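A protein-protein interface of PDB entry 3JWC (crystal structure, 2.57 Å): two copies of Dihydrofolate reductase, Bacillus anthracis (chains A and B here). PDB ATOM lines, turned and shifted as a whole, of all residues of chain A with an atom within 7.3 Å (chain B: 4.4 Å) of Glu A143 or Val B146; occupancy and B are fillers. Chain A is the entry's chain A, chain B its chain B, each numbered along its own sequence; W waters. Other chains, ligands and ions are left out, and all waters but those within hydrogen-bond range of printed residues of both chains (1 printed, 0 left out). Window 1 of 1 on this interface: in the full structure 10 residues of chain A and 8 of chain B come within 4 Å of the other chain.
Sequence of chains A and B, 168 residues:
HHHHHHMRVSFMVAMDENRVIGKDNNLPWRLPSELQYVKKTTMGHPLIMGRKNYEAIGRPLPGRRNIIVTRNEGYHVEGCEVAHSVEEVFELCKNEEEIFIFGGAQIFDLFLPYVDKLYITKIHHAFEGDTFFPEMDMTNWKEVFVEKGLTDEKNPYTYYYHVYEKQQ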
ATOM      1  N   LYS A 122     -32.357  27.964 -14.363  1.00  0.00           N
ATOM      2  CA  LYS A 122     -33.273  27.419 -13.372  1.00  0.00           C
ATOM      3  C   LYS A 122     -33.828  28.509 -12.470  1.00  0.00           C
ATOM      4  O   LYS A 122     -33.086  29.155 -11.725  1.00  0.00           O
ATOM      5  CB  LYS A 122     -32.586  26.350 -12.526  1.00  0.00           C
ATOM      6  CG  LYS A 122     -32.611  24.964 -13.147  1.00  0.00           C
ATOM      7  CD  LYS A 122     -31.319  24.229 -12.843  1.00  0.00           C
ATOM      8  CE  LYS A 122     -31.304  22.860 -13.465  1.00  0.00           C
ATOM      9  NZ  LYS A 122     -30.016  22.230 -13.136  1.00  0.00           N
ATOM     10  N   MET A 138     -28.983  12.711 -17.136  1.00  0.00           N
ATOM     11  CA  MET A 138     -27.752  13.495 -17.132  1.00  0.00           C
ATOM     12  C   MET A 138     -26.489  12.642 -16.987  1.00  0.00           C
ATOM     13  O   MET A 138     -25.383  13.180 -16.899  1.00  0.00           O
ATOM     14  CB  MET A 138     -27.797  14.593 -16.065  1.00  0.00           C
ATOM     15  CG  MET A 138     -28.847  15.678 -16.296  1.00  0.00           C
ATOM     16  SD  MET A 138     -28.860  16.411 -17.950  1.00  0.00           S
ATOM     17  CE  MET A 138     -27.493  17.558 -17.854  1.00  0.00           C
ATOM     18  N   TRP A 141     -23.103  13.672 -18.512  1.00  0.00           N
ATOM     19  CA  TRP A 141     -23.089  15.123 -18.637  1.00  0.00           C
ATOM     20  C   TRP A 141     -22.358  15.726 -17.458  1.00  0.00           C
ATOM     21  O   TRP A 141     -22.494  15.263 -16.329  1.00  0.00           O
ATOM     22  CB  TRP A 141     -24.495  15.703 -18.724  1.00  0.00           C
ATOM     23  CG  TRP A 141     -25.227  15.337 -19.981  1.00  0.00           C
ATOM     24  CD1 TRP A 141     -25.689  14.097 -20.332  1.00  0.00           C
ATOM     25  CD2 TRP A 141     -25.604  16.218 -21.040  1.00  0.00           C
ATOM     26  NE1 TRP A 141     -26.322  14.152 -21.545  1.00  0.00           N
ATOM     27  CE2 TRP A 141     -26.285  15.441 -22.006  1.00  0.00           C
ATOM     28  CE3 TRP A 141     -25.434  17.589 -21.270  1.00  0.00           C
ATOM     29  CZ2 TRP A 141     -26.795  15.988 -23.185  1.00  0.00           C
ATOM     30  CZ3 TRP A 141     -25.941  18.133 -22.439  1.00  0.00           C
ATOM     31  CH2 TRP A 141     -26.616  17.331 -23.381  1.00  0.00           C
ATOM     32  N   LYS A 142     -21.567  16.753 -17.734  1.00  0.00           N
ATOM     33  CA  LYS A 142     -20.868  17.478 -16.688  1.00  0.00           C
ATOM     34  C   LYS A 142     -21.213  18.960 -16.740  1.00  0.00           C
ATOM     35  O   LYS A 142     -21.213  19.574 -17.810  1.00  0.00           O
ATOM     36  CB  LYS A 142     -19.354  17.275 -16.787  1.00  0.00           C
ATOM     37  CG  LYS A 142     -18.924  15.857 -16.494  1.00  0.00           C
ATOM     38  CD  LYS A 142     -17.430  15.754 -16.289  1.00  0.00           C
ATOM     39  CE  LYS A 142     -17.037  14.318 -16.068  1.00  0.00           C
ATOM     40  NZ  LYS A 142     -15.571  14.220 -16.073  1.00  0.00           N
ATOM     41  N   GLU A 143     -21.515  19.523 -15.576  1.00  0.00           N
ATOM     42  CA  GLU A 143     -21.751  20.949 -15.461  1.00  0.00           C
ATOM     43  C   GLU A 143     -20.427  21.672 -15.627  1.00  0.00           C
ATOM     44  O   GLU A 143     -19.460  21.385 -14.918  1.00  0.00           O
ATOM     45  CB  GLU A 143     -22.360  21.272 -14.102  1.00  0.00           C
ATOM     46  CG  GLU A 143     -22.762  22.721 -13.901  1.00  0.00           C
ATOM     47  CD  GLU A 143     -23.322  22.972 -12.513  1.00  0.00           C
ATOM     48  OE1 GLU A 143     -24.540  23.210 -12.400  1.00  0.00           O
ATOM     49  OE2 GLU A 143     -22.552  22.910 -11.530  1.00  0.00           O
ATOM     50  N   VAL A 144     -20.379  22.603 -16.573  1.00  0.00           N
ATOM     51  CA  VAL A 144     -19.137  23.340 -16.838  1.00  0.00           C
ATOM     52  C   VAL A 144     -19.243  24.816 -16.481  1.00  0.00           C
ATOM     53  O   VAL A 144     -18.248  25.538 -16.509  1.00  0.00           O
ATOM     54  CB  VAL A 144     -18.627  23.162 -18.290  1.00  0.00           C
ATOM     55  CG1 VAL A 144     -18.359  21.684 -18.574  1.00  0.00           C
ATOM     56  CG2 VAL A 144     -19.608  23.745 -19.287  1.00  0.00           C
ATOM     57  N   PHE A 145     -20.448  25.255 -16.138  1.00  0.00           N
ATOM     58  CA  PHE A 145     -20.682  26.640 -15.734  1.00  0.00           C
ATOM     59  C   PHE A 145     -21.913  26.747 -14.846  1.00  0.00           C
ATOM     60  O   PHE A 145     -22.928  26.106 -15.106  1.00  0.00           O
ATOM     61  CB  PHE A 145     -20.855  27.549 -16.963  1.00  0.00           C
ATOM     62  CG  PHE A 145     -21.025  29.007 -16.628  1.00  0.00           C
ATOM     63  CD1 PHE A 145     -19.913  29.825 -16.435  1.00  0.00           C
ATOM     64  CD2 PHE A 145     -22.298  29.564 -16.502  1.00  0.00           C
ATOM     65  CE1 PHE A 145     -20.067  31.175 -16.119  1.00  0.00           C
ATOM     66  CE2 PHE A 145     -22.464  30.917 -16.183  1.00  0.00           C
ATOM     67  CZ  PHE A 145     -21.344  31.723 -15.992  1.00  0.00           C
ATOM     68  N   VAL A 146     -21.807  27.566 -13.804  1.00  0.00           N
ATOM     69  CA  VAL A 146     -22.948  27.931 -12.960  1.00  0.00           C
ATOM     70  C   VAL A 146     -22.734  29.307 -12.312  1.00  0.00           C
ATOM     71  O   VAL A 146     -21.653  29.596 -11.786  1.00  0.00           O
ATOM     72  CB  VAL A 146     -23.273  26.838 -11.896  1.00  0.00           C
ATOM     73  CG1 VAL A 146     -22.095  26.605 -10.948  1.00  0.00           C
ATOM     74  CG2 VAL A 146     -24.556  27.179 -11.125  1.00  0.00           C
ATOM     75  N   GLU A 147     -23.763  30.153 -12.367  1.00  0.00           N
ATOM     76  CA  GLU A 147     -23.692  31.512 -11.803  1.00  0.00           C
ATOM     77  C   GLU A 147     -25.084  32.042 -11.448  1.00  0.00           C
ATOM     78  O   GLU A 147     -26.050  31.795 -12.176  1.00  0.00           O
ATOM     79  CB  GLU A 147     -23.006  32.450 -12.794  1.00  0.00           C
ATOM     80  CG  GLU A 147     -22.684  33.819 -12.252  1.00  0.00           C
ATOM     81  CD  GLU A 147     -22.016  34.692 -13.291  1.00  0.00           C
ATOM     82  OE1 GLU A 147     -20.823  34.452 -13.602  1.00  0.00           O
ATOM     83  OE2 GLU A 147     -22.687  35.618 -13.799  1.00  0.00           O
ATOM     84  N   TYR A 161     -27.936  30.468 -13.915  1.00  0.00           N
ATOM     85  CA  TYR A 161     -27.517  29.997 -15.222  1.00  0.00           C
ATOM     86  C   TYR A 161     -26.679  28.740 -15.046  1.00  0.00           C
ATOM     87  O   TYR A 161     -25.709  28.747 -14.289  1.00  0.00           O
ATOM     88  CB  TYR A 161     -26.672  31.061 -15.911  1.00  0.00           C
ATOM     89  CG  TYR A 161     -27.358  32.395 -16.076  1.00  0.00           C
ATOM     90  CD1 TYR A 161     -26.886  33.529 -15.415  1.00  0.00           C
ATOM     91  CD2 TYR A 161     -28.478  32.529 -16.898  1.00  0.00           C
ATOM     92  CE1 TYR A 161     -27.512  34.763 -15.570  1.00  0.00           C
ATOM     93  CE2 TYR A 161     -29.104  33.755 -17.061  1.00  0.00           C
ATOM     94  CZ  TYR A 161     -28.614  34.866 -16.396  1.00  0.00           C
ATOM     95  OH  TYR A 161     -29.240  36.070 -16.554  1.00  0.00           O
ATOM     96  N   HIS A 162     -27.061  27.669 -15.734  1.00  0.00           N
ATOM     97  CA  HIS A 162     -26.297  26.422 -15.746  1.00  0.00           C
ATOM     98  C   HIS A 162     -25.921  26.068 -17.176  1.00  0.00           C
ATOM     99  O   HIS A 162     -26.699  26.290 -18.100  1.00  0.00           O
ATOM    100  CB  HIS A 162     -27.122  25.262 -15.182  1.00  0.00           C
ATOM    101  CG  HIS A 162     -27.559  25.444 -13.764  1.00  0.00           C
ATOM    102  ND1 HIS A 162     -26.953  24.797 -12.710  1.00  0.00           N
ATOM    103  CD2 HIS A 162     -28.566  26.174 -13.227  1.00  0.00           C
ATOM    104  CE1 HIS A 162     -27.553  25.136 -11.582  1.00  0.00           C
ATOM    105  NE2 HIS A 162     -28.541  25.965 -11.869  1.00  0.00           N
ATOM    106  N   VAL A 163     -24.730  25.506 -17.350  1.00  0.00           N
ATOM    107  CA  VAL A 163     -24.311  24.956 -18.635  1.00  0.00           C
ATOM    108  C   VAL A 163     -23.774  23.544 -18.420  1.00  0.00           C
ATOM    109  O   VAL A 163     -22.892  23.321 -17.581  1.00  0.00           O
ATOM    110  CB  VAL A 163     -23.256  25.854 -19.356  1.00  0.00           C
ATOM    111  CG1 VAL A 163     -22.805  25.243 -20.692  1.00  0.00           C
ATOM    112  CG2 VAL A 163     -23.814  27.256 -19.583  1.00  0.00           C
ATOM    113  N   TYR A 164     -24.327  22.593 -19.169  1.00  0.00           N
ATOM    114  CA  TYR A 164     -23.868  21.217 -19.135  1.00  0.00           C
ATOM    115  C   TYR A 164     -23.327  20.795 -20.492  1.00  0.00           C
ATOM    116  O   TYR A 164     -23.830  21.234 -21.522  1.00  0.00           O
ATOM    117  CB  TYR A 164     -25.013  20.284 -18.751  1.00  0.00           C
ATOM    118  CG  TYR A 164     -25.649  20.567 -17.416  1.00  0.00           C
ATOM    119  CD1 TYR A 164     -25.166  19.971 -16.247  1.00  0.00           C
ATOM    120  CD2 TYR A 164     -26.753  21.415 -17.320  1.00  0.00           C
ATOM    121  CE1 TYR A 164     -25.761  20.225 -15.013  1.00  0.00           C
ATOM    122  CE2 TYR A 164     -27.357  21.671 -16.104  1.00  0.00           C
ATOM    123  CZ  TYR A 164     -26.860  21.075 -14.954  1.00  0.00           C
ATOM    124  OH  TYR A 164     -27.468  21.343 -13.753  1.00  0.00           O
ATOM    125  N   GLU A 165     -22.311  19.936 -20.482  1.00  0.00           N
ATOM    126  CA  GLU A 165     -21.776  19.338 -21.705  1.00  0.00           C
ATOM    127  C   GLU A 165     -21.808  17.816 -21.655  1.00  0.00           C
ATOM    128  O   GLU A 165     -21.451  17.215 -20.645  1.00  0.00           O
ATOM    129  CB  GLU A 165     -20.334  19.786 -21.945  1.00  0.00           C
ATOM    130  CG  GLU A 165     -20.172  21.231 -22.346  1.00  0.00           C
ATOM    131  CD  GLU A 165     -18.731  21.588 -22.695  1.00  0.00           C
ATOM    132  OE1 GLU A 165     -17.824  20.741 -22.507  1.00  0.00           O
ATOM    133  OE2 GLU A 165     -18.508  22.726 -23.165  1.00  0.00           O
ATOM    134  N   GLN A 167     -20.465  14.213 -22.262  1.00  0.00           N
ATOM    135  CA  GLN A 167     -19.153  13.561 -22.383  1.00  0.00           C
ATOM    136  C   GLN A 167     -19.165  12.493 -23.479  1.00  0.00           C
ATOM    137  O   GLN A 167     -18.341  12.534 -24.392  1.00  0.00           O
ATOM    138  CB  GLN A 167     -18.684  12.970 -21.049  1.00  0.00           C
ATOM    139  CG  GLN A 167     -18.679  13.957 -19.888  1.00  0.00           C
ATOM    140  CD  GLN A 167     -17.820  15.189 -20.140  1.00  0.00           C
ATOM    141  OE1 GLN A 167     -16.594  15.107 -20.195  1.00  0.00           O
ATOM    142  NE2 GLN A 167     -18.469  16.342 -20.274  1.00  0.00           N
ATOM    143  N   GLU B 143     -16.137   9.112 -13.651  1.00  0.00           N
ATOM    144  CA  GLU B 143     -17.102  10.133 -13.263  1.00  0.00           C
ATOM    145  C   GLU B 143     -18.085  10.376 -14.411  1.00  0.00           C
ATOM    146  O   GLU B 143     -17.686  10.774 -15.511  1.00  0.00           O
ATOM    147  CB  GLU B 143     -16.403  11.442 -12.887  1.00  0.00           C
ATOM    148  CG  GLU B 143     -17.319  12.453 -12.162  1.00  0.00           C
ATOM    149  CD  GLU B 143     -16.642  13.786 -11.882  1.00  0.00           C
ATOM    150  OE1 GLU B 143     -16.692  14.229 -10.718  1.00  0.00           O
ATOM    151  OE2 GLU B 143     -16.055  14.393 -12.811  1.00  0.00           O
ATOM    152  N   PHE B 145     -21.134  12.177 -13.851  1.00  0.00           N
ATOM    153  CA  PHE B 145     -21.925  13.365 -13.542  1.00  0.00           C
ATOM    154  C   PHE B 145     -21.273  14.194 -12.442  1.00  0.00           C
ATOM    155  O   PHE B 145     -20.715  13.644 -11.492  1.00  0.00           O
ATOM    156  CB  PHE B 145     -23.352  12.959 -13.146  1.00  0.00           C
ATOM    157  CG  PHE B 145     -24.280  14.120 -12.916  1.00  0.00           C
ATOM    158  CD1 PHE B 145     -24.743  14.887 -13.980  1.00  0.00           C
ATOM    159  CD2 PHE B 145     -24.701  14.439 -11.633  1.00  0.00           C
ATOM    160  CE1 PHE B 145     -25.606  15.959 -13.773  1.00  0.00           C
ATOM    161  CE2 PHE B 145     -25.569  15.507 -11.415  1.00  0.00           C
ATOM    162  CZ  PHE B 145     -26.024  16.268 -12.492  1.00  0.00           C
ATOM    163  N   VAL B 146     -21.345  15.515 -12.586  1.00  0.00           N
ATOM    164  CA  VAL B 146     -20.915  16.461 -11.550  1.00  0.00           C
ATOM    165  C   VAL B 146     -21.687  17.783 -11.692  1.00  0.00           C
ATOM    166  O   VAL B 146     -21.859  18.290 -12.801  1.00  0.00           O
ATOM    167  CB  VAL B 146     -19.364  16.693 -11.569  1.00  0.00           C
ATOM    168  CG1 VAL B 146     -18.885  17.223 -12.920  1.00  0.00           C
ATOM    169  CG2 VAL B 146     -18.934  17.615 -10.434  1.00  0.00           C
ATOM    170  N   GLU B 147     -22.180  18.313 -10.575  1.00  0.00           N
ATOM    171  CA  GLU B 147     -22.787  19.655 -10.551  1.00  0.00           C
ATOM    172  C   GLU B 147     -22.728  20.300  -9.163  1.00  0.00           C
ATOM    173  O   GLU B 147     -22.769  19.605  -8.135  1.00  0.00           O
ATOM    174  CB  GLU B 147     -24.229  19.654 -11.094  1.00  0.00           C
ATOM    175  CG  GLU B 147     -25.303  19.270 -10.079  1.00  0.00           C
ATOM    176  CD  GLU B 147     -26.726  19.420 -10.603  1.00  0.00           C
ATOM    177  OE1 GLU B 147     -26.908  19.658 -11.811  1.00  0.00           O
ATOM    178  OE2 GLU B 147     -27.673  19.291  -9.794  1.00  0.00           O
ATOM    179  N   LYS B 148     -22.617  21.627  -9.143  1.00  0.00           N
ATOM    180  CA  LYS B 148     -22.578  22.378  -7.897  1.00  0.00           C
ATOM    181  C   LYS B 148     -23.927  22.270  -7.206  1.00  0.00           C
ATOM    182  O   LYS B 148     -24.965  22.377  -7.849  1.00  0.00           O
ATOM    183  CB  LYS B 148     -22.223  23.842  -8.163  1.00  0.00           C
ATOM    184  CG  LYS B 148     -21.785  24.631  -6.937  1.00  0.00           C
ATOM    185  CD  LYS B 148     -21.462  26.082  -7.285  1.00  0.00           C
ATOM    186  CE  LYS B 148     -20.800  26.820  -6.124  1.00  0.00           C
ATOM    187  NZ  LYS B 148     -21.654  26.921  -4.910  1.00  0.00           N
ATOM    188  N   TYR B 161     -22.384  17.528  -6.234  1.00  0.00           N
ATOM    189  CA  TYR B 161     -22.894  16.183  -6.479  1.00  0.00           C
ATOM    190  C   TYR B 161     -21.987  15.493  -7.485  1.00  0.00           C
ATOM    191  O   TYR B 161     -21.754  16.028  -8.569  1.00  0.00           O
ATOM    192  CB  TYR B 161     -24.306  16.222  -7.053  1.00  0.00           C
ATOM    193  CG  TYR B 161     -25.321  16.946  -6.200  1.00  0.00           C
ATOM    194  CD1 TYR B 161     -25.933  18.132  -6.655  1.00  0.00           C
ATOM    195  CD2 TYR B 161     -25.681  16.454  -4.935  1.00  0.00           C
ATOM    196  CE1 TYR B 161     -26.868  18.798  -5.877  1.00  0.00           C
ATOM    197  CE2 TYR B 161     -26.615  17.121  -4.148  1.00  0.00           C
ATOM    198  CZ  TYR B 161     -27.204  18.285  -4.628  1.00  0.00           C
ATOM    199  OH  TYR B 161     -28.123  18.931  -3.840  1.00  0.00           O
ATOM    200  N   HIS B 162     -21.464  14.322  -7.123  1.00  0.00           N
ATOM    201  CA  HIS B 162     -20.668  13.522  -8.043  1.00  0.00           C
ATOM    202  C   HIS B 162     -21.314  12.164  -8.193  1.00  0.00           C
ATOM    203  O   HIS B 162     -21.884  11.632  -7.236  1.00  0.00           O
ATOM    204  CB  HIS B 162     -19.248  13.314  -7.534  1.00  0.00           C
ATOM    205  CG  HIS B 162     -18.450  14.574  -7.365  1.00  0.00           C
ATOM    206  ND1 HIS B 162     -17.488  14.972  -8.269  1.00  0.00           N
ATOM    207  CD2 HIS B 162     -18.430  15.491  -6.368  1.00  0.00           C
ATOM    208  CE1 HIS B 162     -16.926  16.091  -7.849  1.00  0.00           C
ATOM    209  NE2 HIS B 162     -17.477  16.425  -6.695  1.00  0.00           N
HETATM  210  O   HOH W   1     -25.627  23.761  -9.957  1.00  0.00           O
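The side-chain amino group (NZ) of Lys A122 sits at hydrogen-bond distance from the side-chain hydroxyl (OH) of Tyr A164 (2.8 Å).
The backbone NH (N) of Glu A165 lies within hydrogen-bond range of the backbone carbonyl oxygen (O) of Lys A142 (2.9 Å).
OE1 of Glu A143 sits at hydrogen-bond distance from ND1 of His A162.
The side-chain carboxylate of Glu B143 lies within hydrogen-bond range of a ring nitrogen (ND1) of His B162 (2.7 Å).
The backbone carbonyl oxygen of Glu B147 lies within hydrogen-bond range of the backbone NH of Tyr B161 (2.8 Å).
Water W1 lies within hydrogen-bond range of O of Lys B148 (2.6 Å), OE1 of Glu A143 (2.7 Å) and ND1 of His A162 (3.2 Å).
O of Met A138 touches CD1 of Phe B145, at 3.4 Å.
O of Trp A141 touches CD1 of Phe B145, 3.3 Å away.
O of Trp A141 touches N of Val B146, 3.9 Å away.
Val B146 touches Lys A142.
Glu B147 touches Glu A143 (CA to OE2, 3.4 Å).
CD of Lys B148 touches CG1 of Val A146 (3.8 Å).
Tyr A161 touches none of the printed residues of chain B.
Of the printed residues of chain B, Tyr A164 touches Glu B147.
Val B146 touches three residues of chain A.
Of the printed residues of chain A, Lys B148 touches Glu A143 (2.7 Å) and Val A146 (3.8 Å).
The nearest printed residue of chain B that does not touch Glu A143 is Phe B145 (5.7 Å).
Of the 15 printed residues of chain A, 6 touch a printed residue of chain B.
Printed residues of chain A that touch a printed residue of chain B: Met A138, Trp A141, Lys A142, Glu A143, Val A146 and Tyr A164.
Among the printed residues, Asp or Glu carboxylates within 4 Å of a Lys or Arg side-chain nitrogen of the other chain: Lys A142 with Glu B143 (3.3 Å).
The side-chain amino group (NZ) of Lys A142 lies within salt-bridge range of the side-chain carboxylate (OE2) of Glu B143 (3.3 Å).
The backbone NH (N) of Glu A143 sits at hydrogen-bond distance from the backbone carbonyl oxygen (O) of Val B146 (3.1 Å).
The side-chain carboxylate of Glu A143 is in hydrogen-bond range of the backbone NH of Lys B148 (2.7 Å).
OE1 of Glu B147 is in hydrogen-bond range of OH of Tyr A164, 2.6 Å away.
Glu A143 touches Val B146, but with the chains exchanged Val A146 does not touch Glu B143 (13.5 Å).
Glu A143 touches Glu B147, but with the chains exchanged Glu A147 does not touch Glu B143 (17.5 Å).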
